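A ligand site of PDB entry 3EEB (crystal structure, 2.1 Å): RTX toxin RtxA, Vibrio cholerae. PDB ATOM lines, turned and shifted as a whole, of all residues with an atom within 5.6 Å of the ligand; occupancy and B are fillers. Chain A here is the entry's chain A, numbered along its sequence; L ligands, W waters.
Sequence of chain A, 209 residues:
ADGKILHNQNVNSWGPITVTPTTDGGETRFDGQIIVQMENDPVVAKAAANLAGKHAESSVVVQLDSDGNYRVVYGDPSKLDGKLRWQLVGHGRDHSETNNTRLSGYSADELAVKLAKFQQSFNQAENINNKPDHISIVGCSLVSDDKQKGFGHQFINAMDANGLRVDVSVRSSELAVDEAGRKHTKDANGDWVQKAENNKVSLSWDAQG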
ATOM      1  N   GLY A  25      -7.383 -27.357   6.198  1.00  0.00           N
ATOM      2  CA  GLY A  25      -6.390 -26.272   6.132  1.00  0.00           C
ATOM      3  C   GLY A  25      -6.510 -25.181   7.188  1.00  0.00           C
ATOM      4  O   GLY A  25      -5.503 -24.602   7.602  1.00  0.00           O
ATOM      5  N   GLU A  27      -7.537 -21.505   8.988  1.00  0.00           N
ATOM      6  CA  GLU A  27      -7.412 -20.101   8.586  1.00  0.00           C
ATOM      7  C   GLU A  27      -5.947 -19.661   8.435  1.00  0.00           C
ATOM      8  O   GLU A  27      -5.047 -20.193   9.096  1.00  0.00           O
ATOM      9  CB  GLU A  27      -8.141 -19.203   9.578  1.00  0.00           C
ATOM     10  CG  GLU A  27      -9.670 -19.452   9.686  1.00  0.00           C
ATOM     11  CD  GLU A  27     -10.245 -19.084  11.059  1.00  0.00           C
ATOM     12  OE1 GLU A  27      -9.665 -19.512  12.089  1.00  0.00           O
ATOM     13  OE2 GLU A  27     -11.287 -18.371  11.107  1.00  0.00           O
ATOM     14  N   THR A  28      -5.701 -18.699   7.549  1.00  0.00           N
ATOM     15  CA  THR A  28      -4.386 -18.074   7.408  1.00  0.00           C
ATOM     16  C   THR A  28      -4.511 -16.566   7.610  1.00  0.00           C
ATOM     17  O   THR A  28      -5.544 -15.980   7.264  1.00  0.00           O
ATOM     18  CB  THR A  28      -3.737 -18.376   6.031  1.00  0.00           C
ATOM     19  OG1 THR A  28      -2.495 -17.656   5.913  1.00  0.00           O
ATOM     20  CG2 THR A  28      -4.660 -17.974   4.856  1.00  0.00           C
ATOM     21  N   ARG A  29      -3.454 -15.952   8.151  1.00  0.00           N
ATOM     22  CA  ARG A  29      -3.429 -14.493   8.350  1.00  0.00           C
ATOM     23  C   ARG A  29      -3.237 -13.706   7.053  1.00  0.00           C
ATOM     24  O   ARG A  29      -3.409 -12.497   7.034  1.00  0.00           O
ATOM     25  CB  ARG A  29      -2.351 -14.103   9.369  1.00  0.00           C
ATOM     26  CG  ARG A  29      -0.925 -14.450   8.977  1.00  0.00           C
ATOM     27  CD  ARG A  29       0.096 -13.540   9.638  1.00  0.00           C
ATOM     28  NE  ARG A  29       1.426 -14.140   9.671  1.00  0.00           N
ATOM     29  CZ  ARG A  29       2.573 -13.464   9.639  1.00  0.00           C
ATOM     30  NH1 ARG A  29       2.569 -12.142   9.559  1.00  0.00           N
ATOM     31  NH2 ARG A  29       3.727 -14.132   9.669  1.00  0.00           N
ATOM     32  N   PHE A  30      -2.862 -14.408   5.983  1.00  0.00           N
ATOM     33  CA  PHE A  30      -2.669 -13.784   4.682  1.00  0.00           C
ATOM     34  C   PHE A  30      -3.940 -13.878   3.852  1.00  0.00           C
ATOM     35  O   PHE A  30      -4.544 -14.939   3.723  1.00  0.00           O
ATOM     36  CB  PHE A  30      -1.458 -14.386   3.957  1.00  0.00           C
ATOM     37  CG  PHE A  30      -0.186 -14.276   4.745  1.00  0.00           C
ATOM     38  CD1 PHE A  30       0.527 -13.087   4.770  1.00  0.00           C
ATOM     39  CD2 PHE A  30       0.280 -15.356   5.490  1.00  0.00           C
ATOM     40  CE1 PHE A  30       1.696 -12.970   5.529  1.00  0.00           C
ATOM     41  CE2 PHE A  30       1.460 -15.259   6.251  1.00  0.00           C
ATOM     42  CZ  PHE A  30       2.167 -14.074   6.270  1.00  0.00           C
ATOM     43  N   LYS A  54      -3.581 -26.302   0.699  1.00  0.00           N
ATOM     44  CA  LYS A  54      -3.921 -25.890   2.066  1.00  0.00           C
ATOM     45  C   LYS A  54      -4.815 -24.652   2.116  1.00  0.00           C
ATOM     46  O   LYS A  54      -5.738 -24.569   2.939  1.00  0.00           O
ATOM     47  CB  LYS A  54      -2.658 -25.645   2.914  1.00  0.00           C
ATOM     48  CG  LYS A  54      -2.858 -25.951   4.399  1.00  0.00           C
ATOM     49  CD  LYS A  54      -1.943 -25.148   5.315  1.00  0.00           C
ATOM     50  CE  LYS A  54      -2.178 -25.527   6.774  1.00  0.00           C
ATOM     51  NZ  LYS A  54      -1.249 -24.784   7.684  1.00  0.00           N
ATOM     52  N   HIS A  55      -4.532 -23.685   1.238  1.00  0.00           N
ATOM     53  CA  HIS A  55      -5.350 -22.483   1.121  1.00  0.00           C
ATOM     54  C   HIS A  55      -5.735 -22.209  -0.342  1.00  0.00           C
ATOM     55  O   HIS A  55      -5.457 -21.149  -0.882  1.00  0.00           O
ATOM     56  CB  HIS A  55      -4.640 -21.272   1.749  1.00  0.00           C
ATOM     57  CG  HIS A  55      -4.317 -21.442   3.205  1.00  0.00           C
ATOM     58  ND1 HIS A  55      -5.295 -21.582   4.172  1.00  0.00           N
ATOM     59  CD2 HIS A  55      -3.135 -21.514   3.858  1.00  0.00           C
ATOM     60  CE1 HIS A  55      -4.719 -21.724   5.359  1.00  0.00           C
ATOM     61  NE2 HIS A  55      -3.411 -21.687   5.183  1.00  0.00           N
ATOM     62  N   ARG A  85       1.546 -13.198   1.384  1.00  0.00           N
ATOM     63  CA  ARG A  85       2.740 -14.001   1.640  1.00  0.00           C
ATOM     64  C   ARG A  85       3.289 -14.574   0.328  1.00  0.00           C
ATOM     65  O   ARG A  85       2.536 -14.845  -0.603  1.00  0.00           O
ATOM     66  CB  ARG A  85       2.424 -15.136   2.622  1.00  0.00           C
ATOM     67  CG  ARG A  85       3.607 -16.093   2.848  1.00  0.00           C
ATOM     68  CD  ARG A  85       3.318 -17.145   3.889  1.00  0.00           C
ATOM     69  NE  ARG A  85       2.067 -17.832   3.620  1.00  0.00           N
ATOM     70  CZ  ARG A  85       1.480 -18.696   4.446  1.00  0.00           C
ATOM     71  NH1 ARG A  85       2.017 -18.985   5.625  1.00  0.00           N
ATOM     72  NH2 ARG A  85       0.333 -19.251   4.088  1.00  0.00           N
ATOM     73  N   GLN A  87       5.569 -17.927  -0.617  1.00  0.00           N
ATOM     74  CA  GLN A  87       6.298 -19.125  -0.209  1.00  0.00           C
ATOM     75  C   GLN A  87       7.206 -19.607  -1.341  1.00  0.00           C
ATOM     76  O   GLN A  87       6.726 -20.036  -2.398  1.00  0.00           O
ATOM     77  CB  GLN A  87       5.364 -20.249   0.277  1.00  0.00           C
ATOM     78  CG  GLN A  87       4.342 -19.828   1.328  1.00  0.00           C
ATOM     79  CD  GLN A  87       3.926 -20.969   2.243  1.00  0.00           C
ATOM     80  OE1 GLN A  87       4.778 -21.621   2.843  1.00  0.00           O
ATOM     81  NE2 GLN A  87       2.616 -21.197   2.358  1.00  0.00           N
ATOM     82  N   HIS A 134       5.516 -10.932   3.710  1.00  0.00           N
ATOM     83  CA  HIS A 134       6.249 -12.061   4.267  1.00  0.00           C
ATOM     84  C   HIS A 134       6.710 -12.996   3.172  1.00  0.00           C
ATOM     85  O   HIS A 134       5.996 -13.201   2.178  1.00  0.00           O
ATOM     86  CB  HIS A 134       5.365 -12.840   5.258  1.00  0.00           C
ATOM     87  CG  HIS A 134       6.098 -13.876   6.042  1.00  0.00           C
ATOM     88  ND1 HIS A 134       6.555 -13.648   7.321  1.00  0.00           N
ATOM     89  CD2 HIS A 134       6.469 -15.134   5.726  1.00  0.00           C
ATOM     90  CE1 HIS A 134       7.167 -14.728   7.765  1.00  0.00           C
ATOM     91  NE2 HIS A 134       7.128 -15.651   6.814  1.00  0.00           N
ATOM     92  N   SER A 136       8.054 -16.885   3.114  1.00  0.00           N
ATOM     93  CA  SER A 136       8.379 -18.137   3.752  1.00  0.00           C
ATOM     94  C   SER A 136       9.307 -18.926   2.838  1.00  0.00           C
ATOM     95  O   SER A 136       8.933 -19.292   1.717  1.00  0.00           O
ATOM     96  CB  SER A 136       7.122 -18.933   4.066  1.00  0.00           C
ATOM     97  OG  SER A 136       7.480 -20.088   4.779  1.00  0.00           O
ATOM     98  N   SER A 169      10.663 -16.036   6.986  1.00  0.00           N
ATOM     99  CA  SER A 169      10.824 -17.259   7.758  1.00  0.00           C
ATOM    100  C   SER A 169      11.679 -18.256   6.979  1.00  0.00           C
ATOM    101  O   SER A 169      11.526 -18.405   5.759  1.00  0.00           O
ATOM    102  CB  SER A 169       9.471 -17.860   8.160  1.00  0.00           C
ATOM    103  OG  SER A 169       8.585 -17.872   7.058  1.00  0.00           O
ATOM    104  N   ARG A 171      14.316 -22.045   7.367  1.00  0.00           N
ATOM    105  CA  ARG A 171      14.627 -23.212   8.176  1.00  0.00           C
ATOM    106  C   ARG A 171      16.114 -23.563   8.164  1.00  0.00           C
ATOM    107  O   ARG A 171      16.789 -23.456   7.139  1.00  0.00           O
ATOM    108  CB  ARG A 171      13.808 -24.414   7.732  1.00  0.00           C
ATOM    109  CG  ARG A 171      12.343 -24.293   8.046  1.00  0.00           C
ATOM    110  CD  ARG A 171      11.617 -23.454   7.002  1.00  0.00           C
ATOM    111  NE  ARG A 171      10.226 -23.245   7.373  1.00  0.00           N
ATOM    112  CZ  ARG A 171       9.418 -22.355   6.794  1.00  0.00           C
ATOM    113  NH1 ARG A 171       9.843 -21.598   5.794  1.00  0.00           N
ATOM    114  NH2 ARG A 171       8.179 -22.245   7.219  1.00  0.00           N
ATOM    115  N   GLY A 181      -0.130 -30.032   2.812  1.00  0.00           N
ATOM    116  CA  GLY A 181       0.593 -28.762   2.658  1.00  0.00           C
ATOM    117  C   GLY A 181       1.200 -28.259   3.956  1.00  0.00           C
ATOM    118  O   GLY A 181       1.395 -27.044   4.117  1.00  0.00           O
ATOM    119  N   ARG A 182       1.491 -29.184   4.873  1.00  0.00           N
ATOM    120  CA  ARG A 182       2.107 -28.852   6.164  1.00  0.00           C
ATOM    121  C   ARG A 182       3.592 -29.162   6.159  1.00  0.00           C
ATOM    122  O   ARG A 182       4.008 -30.192   5.614  1.00  0.00           O
ATOM    123  CB  ARG A 182       1.401 -29.587   7.307  1.00  0.00           C
ATOM    124  CG  ARG A 182       0.007 -29.024   7.582  1.00  0.00           C
ATOM    125  CD  ARG A 182      -0.661 -29.689   8.765  1.00  0.00           C
ATOM    126  NE  ARG A 182      -1.952 -29.049   9.016  1.00  0.00           N
ATOM    127  CZ  ARG A 182      -3.133 -29.607   8.766  1.00  0.00           C
ATOM    128  NH1 ARG A 182      -3.194 -30.841   8.282  1.00  0.00           N
ATOM    129  NH2 ARG A 182      -4.252 -28.933   9.015  1.00  0.00           N
ATOM    130  N   LYS A 183       4.390 -28.291   6.767  1.00  0.00           N
ATOM    131  CA  LYS A 183       5.842 -28.464   6.827  1.00  0.00           C
ATOM    132  C   LYS A 183       6.266 -29.478   7.870  1.00  0.00           C
ATOM    133  O   LYS A 183       5.668 -29.568   8.948  1.00  0.00           O
ATOM    134  CB  LYS A 183       6.554 -27.133   7.110  1.00  0.00           C
ATOM    135  CG  LYS A 183       6.679 -26.224   5.904  1.00  0.00           C
ATOM    136  CD  LYS A 183       5.670 -25.109   5.989  1.00  0.00           C
ATOM    137  CE  LYS A 183       5.792 -24.119   4.841  1.00  0.00           C
ATOM    138  NZ  LYS A 183       4.700 -23.079   5.004  1.00  0.00           N
ATOM    139  N   HIS A 184       7.311 -30.231   7.544  1.00  0.00           N
ATOM    140  CA  HIS A 184       7.965 -31.132   8.469  1.00  0.00           C
ATOM    141  C   HIS A 184       9.458 -30.838   8.457  1.00  0.00           C
ATOM    142  O   HIS A 184      10.040 -30.589   7.401  1.00  0.00           O
ATOM    143  CB  HIS A 184       7.752 -32.589   8.054  1.00  0.00           C
ATOM    144  CG  HIS A 184       6.327 -33.047   8.164  1.00  0.00           C
ATOM    145  ND1 HIS A 184       5.928 -34.033   9.042  1.00  0.00           N
ATOM    146  CD2 HIS A 184       5.206 -32.648   7.507  1.00  0.00           C
ATOM    147  CE1 HIS A 184       4.616 -34.218   8.923  1.00  0.00           C
ATOM    148  NE2 HIS A 184       4.159 -33.381   8.005  1.00  0.00           N
ATOM    149  N   GLN A 194       6.812 -32.094  13.379  1.00  0.00           N
ATOM    150  CA  GLN A 194       6.031 -30.906  13.010  1.00  0.00           C
ATOM    151  C   GLN A 194       6.159 -29.801  14.052  1.00  0.00           C
ATOM    152  O   GLN A 194       6.304 -30.087  15.233  1.00  0.00           O
ATOM    153  CB  GLN A 194       4.567 -31.271  12.814  1.00  0.00           C
ATOM    154  CG  GLN A 194       4.346 -32.171  11.612  1.00  0.00           C
ATOM    155  CD  GLN A 194       2.893 -32.471  11.395  1.00  0.00           C
ATOM    156  OE1 GLN A 194       2.153 -31.632  10.859  1.00  0.00           O
ATOM    157  NE2 GLN A 194       2.474 -33.664  11.805  1.00  0.00           N
ATOM    158  N   LYS A 195       6.094 -28.561  13.584  1.00  0.00           N
ATOM    159  CA  LYS A 195       6.275 -27.349  14.420  1.00  0.00           C
ATOM    160  C   LYS A 195       7.416 -27.484  15.437  1.00  0.00           C
ATOM    161  O   LYS A 195       7.241 -27.324  16.655  1.00  0.00           O
ATOM    162  CB  LYS A 195       4.958 -26.938  15.107  1.00  0.00           C
ATOM    163  CG  LYS A 195       3.723 -27.056  14.244  1.00  0.00           C
ATOM    164  CD  LYS A 195       2.606 -26.192  14.794  1.00  0.00           C
ATOM    165  CE  LYS A 195       1.374 -26.199  13.890  1.00  0.00           C
ATOM    166  NZ  LYS A 195       1.700 -25.698  12.526  1.00  0.00           N
ATOM    167  N   GLU A 197      10.248 -25.533  16.541  1.00  0.00           N
ATOM    168  CA  GLU A 197      10.601 -24.105  16.439  1.00  0.00           C
ATOM    169  C   GLU A 197      12.099 -23.837  16.392  1.00  0.00           C
ATOM    170  O   GLU A 197      12.543 -22.794  15.888  1.00  0.00           O
ATOM    171  CB  GLU A 197       9.930 -23.285  17.560  1.00  0.00           C
ATOM    172  CG  GLU A 197       8.392 -23.346  17.590  1.00  0.00           C
ATOM    173  CD  GLU A 197       7.741 -22.765  16.321  1.00  0.00           C
ATOM    174  OE1 GLU A 197       8.275 -21.786  15.758  1.00  0.00           O
ATOM    175  OE2 GLU A 197       6.671 -23.277  15.909  1.00  0.00           O
ATOM    176  N   LYS A 200      13.451 -23.399  12.717  1.00  0.00           N
ATOM    177  CA  LYS A 200      13.051 -22.256  11.916  1.00  0.00           C
ATOM    178  C   LYS A 200      13.311 -20.956  12.669  1.00  0.00           C
ATOM    179  O   LYS A 200      13.345 -20.967  13.889  1.00  0.00           O
ATOM    180  CB  LYS A 200      11.568 -22.353  11.526  1.00  0.00           C
ATOM    181  CG  LYS A 200      11.028 -21.149  10.728  1.00  0.00           C
ATOM    182  CD  LYS A 200       9.587 -21.362  10.282  1.00  0.00           C
ATOM    183  CE  LYS A 200       8.566 -20.820  11.257  1.00  0.00           C
ATOM    184  NZ  LYS A 200       7.203 -20.860  10.661  1.00  0.00           N
ATOM    185  N   SER A 202      12.069 -16.648  12.282  1.00  0.00           N
ATOM    186  CA  SER A 202      11.380 -15.565  11.577  1.00  0.00           C
ATOM    187  C   SER A 202      12.243 -14.318  11.711  1.00  0.00           C
ATOM    188  O   SER A 202      12.440 -13.801  12.813  1.00  0.00           O
ATOM    189  CB  SER A 202       9.991 -15.294  12.147  1.00  0.00           C
ATOM    190  OG  SER A 202       9.148 -16.433  12.063  1.00  0.00           O
HETATM  191  C1  LIG L   1       1.151 -22.561   9.984  1.00  0.00           C
HETATM  192  C2  LIG L   1       1.018 -21.198   9.323  1.00  0.00           C
HETATM  193  C3  LIG L   1       2.340 -20.448   9.427  1.00  0.00           C
HETATM  194  C4  LIG L   1       3.500 -21.249   8.798  1.00  0.00           C
HETATM  195  C5  LIG L   1       3.587 -22.606   9.513  1.00  0.00           C
HETATM  196  C6  LIG L   1       2.278 -23.361   9.340  1.00  0.00           C
HETATM  197  O1  LIG L   1      -0.054 -23.276   9.838  1.00  0.00           O
HETATM  198  P1  LIG L   1      -1.135 -23.419  11.039  1.00  0.00           P
HETATM  199  O2  LIG L   1      -2.035 -24.493  10.472  1.00  0.00           O
HETATM  200  O3  LIG L   1      -1.748 -22.053  11.152  1.00  0.00           O
HETATM  201  O4  LIG L   1      -0.360 -23.828  12.251  1.00  0.00           O
HETATM  202  O5  LIG L   1       0.705 -21.369   7.950  1.00  0.00           O
HETATM  203  P2  LIG L   1      -0.720 -20.932   7.326  1.00  0.00           P
HETATM  204  O6  LIG L   1      -0.835 -21.852   6.157  1.00  0.00           O
HETATM  205  O7  LIG L   1      -1.684 -21.223   8.448  1.00  0.00           O
HETATM  206  O8  LIG L   1      -0.625 -19.459   7.015  1.00  0.00           O
HETATM  207  O9  LIG L   1       2.189 -19.172   8.822  1.00  0.00           O
HETATM  208  P3  LIG L   1       2.593 -17.839   9.615  1.00  0.00           P
HETATM  209  O10 LIG L   1       3.570 -17.151   8.685  1.00  0.00           O
HETATM  210  O11 LIG L   1       3.187 -18.367  10.905  1.00  0.00           O
HETATM  211  O12 LIG L   1       1.307 -17.054   9.742  1.00  0.00           O
HETATM  212  O13 LIG L   1       4.693 -20.484   8.939  1.00  0.00           O
HETATM  213  P4  LIG L   1       5.514 -19.886   7.684  1.00  0.00           P
HETATM  214  O14 LIG L   1       4.638 -18.789   7.130  1.00  0.00           O
HETATM  215  O15 LIG L   1       6.823 -19.414   8.273  1.00  0.00           O
HETATM  216  O16 LIG L   1       5.747 -21.094   6.776  1.00  0.00           O
HETATM  217  O17 LIG L   1       4.659 -23.418   9.018  1.00  0.00           O
HETATM  218  P5  LIG L   1       5.748 -24.092   9.983  1.00  0.00           P
HETATM  219  O18 LIG L   1       5.631 -23.332  11.270  1.00  0.00           O
HETATM  220  O19 LIG L   1       5.416 -25.556  10.118  1.00  0.00           O
HETATM  221  O20 LIG L   1       7.031 -23.813   9.230  1.00  0.00           O
HETATM  222  O21 LIG L   1       2.335 -24.667   9.916  1.00  0.00           O
HETATM  223  P6  LIG L   1       2.159 -26.010   9.036  1.00  0.00           P
HETATM  224  O22 LIG L   1       3.530 -26.442   8.597  1.00  0.00           O
HETATM  225  O23 LIG L   1       1.528 -26.982  10.016  1.00  0.00           O
HETATM  226  O24 LIG L   1       1.289 -25.628   7.869  1.00  0.00           O
HETATM  227  O   HOH W   1       2.336 -24.791   5.295  1.00  0.00           O
HETATM  228  O   HOH W   2       6.552 -27.782  10.934  1.00  0.00           O
HETATM  229  O   HOH W   3       4.440 -16.592  13.514  1.00  0.00           O
HETATM  230  O   HOH W   4       1.214 -22.693   4.770  1.00  0.00           O
HETATM  231  O   HOH W   5      -2.306 -19.008  10.821  1.00  0.00           O
HETATM  232  O   HOH W   6      -0.338 -19.781  12.528  1.00  0.00           O
HETATM  233  O   HOH W   7       6.146 -17.688  10.264  1.00  0.00           O
HETATM  234  O   HOH W   8       9.208 -25.009   9.354  1.00  0.00           O
HETATM  235  O   HOH W   9      -0.928 -26.858  10.620  1.00  0.00           O
HETATM  236  O   HOH W  10       7.456 -24.510  12.956  1.00  0.00           O
HETATM  237  O   HOH W  11      -4.242 -23.224   9.685  1.00  0.00           O
HETATM  238  O   HOH W  12      -0.872 -17.725   8.690  1.00  0.00           O
HETATM  239  O   HOH W  13       3.264 -29.055  10.540  1.00  0.00           O
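An oxygen (O15) of the ligand sits at hydrogen-bond distance from the side-chain hydroxyl (OG) of Ser 169, 2.6 Å away.
The side-chain amino group (NZ) of Lys 54 is in salt-bridge range of an oxygen (O24) of the ligand, 2.7 Å away.
NH2 of Arg 171 is in salt-bridge range of O16 of the ligand, 2.7 Å away.
N of Lys 183 sits at hydrogen-bond distance from O22 of the ligand.
NZ of Lys 183 lies within salt-bridge range of O16 of the ligand, at 2.9 Å.
A ring nitrogen (NE2) of His 55 lies within hydrogen-bond range of an oxygen (O6) of the ligand (2.8 Å).
An oxygen (O4) of the ligand lies within salt-bridge range of the side-chain amino group (NZ) of Lys 195 (2.8 Å).
O15 of the ligand lies within salt-bridge range of NZ of Lys 200.
An oxygen (O8) of the ligand sits at hydrogen-bond distance from the side-chain hydroxyl of Thr 28 (2.8 Å).
The side-chain hydroxyl (OG) of Ser 136 sits at hydrogen-bond distance from an oxygen (O16) of the ligand, at 2.8 Å.
An oxygen (O12) of the ligand lies within salt-bridge range of the guanidinium group (NE) of Arg 29, 2.9 Å away.
The guanidinium group of Arg 85 is in salt-bridge range of an oxygen (O8) of the ligand, at 3.0 Å.
The side-chain hydroxyl of Ser 136 lies close to the side-chain hydroxyl of Ser 169 (3.4 Å).
NE2 of His 134 is in hydrogen-bond range of OG of Ser 169 (2.7 Å).
The side-chain hydroxyl (OG) of Ser 136 is in hydrogen-bond range of the guanidinium group (NH1) of Arg 171 (3.0 Å).
The side-chain amide oxygen (OE1) of Gln 87 is in hydrogen-bond range of the side-chain amino group (NZ) of Lys 183.
N of Phe 30 lies close to OG1 of Thr 28 (3.3 Å).
The guanidinium group of Arg 85 sits close to the side-chain amide nitrogen of Gln 87.
Merely in contact with the ligand: Arg 182 (3.5 Å), Glu 27 (3.6 Å) and Phe 30 (3.7 Å).
Hydrophobic or aromatic side chains within 4 Å of the ligand: Phe 30 and His 55.
Water W12 lies within hydrogen-bond range of O8 of the ligand (2.4 Å), N of Arg 29 (3.2 Å) and OG1 of Thr 28 (3.2 Å).
Water W8 bridges an oxygen (O20) of the ligand (2.5 Å) and the guanidinium group of Arg 171 (2.8 Å).
Water W2 lies within hydrogen-bond range of an oxygen (O19) of the ligand (2.6 Å), the backbone NH (N) of Lys 195 (2.8 Å) and the backbone carbonyl oxygen (O) of Lys 183 (2.8 Å).
Water W11 lies within hydrogen-bond range of O2 of the ligand (2.7 Å), O of Gly 25 (2.8 Å) and O of Glu 27 (3.2 Å).
Water W10 lies within hydrogen-bond range of an oxygen (O18) of the ligand (2.7 Å) and the side-chain carboxylate of Glu 197 (3.3 Å).
Water W1 lies within hydrogen-bond range of O of Gly 181 (2.7 Å), O24 of the ligand (2.9 Å) and NZ of Lys 183 (2.9 Å).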
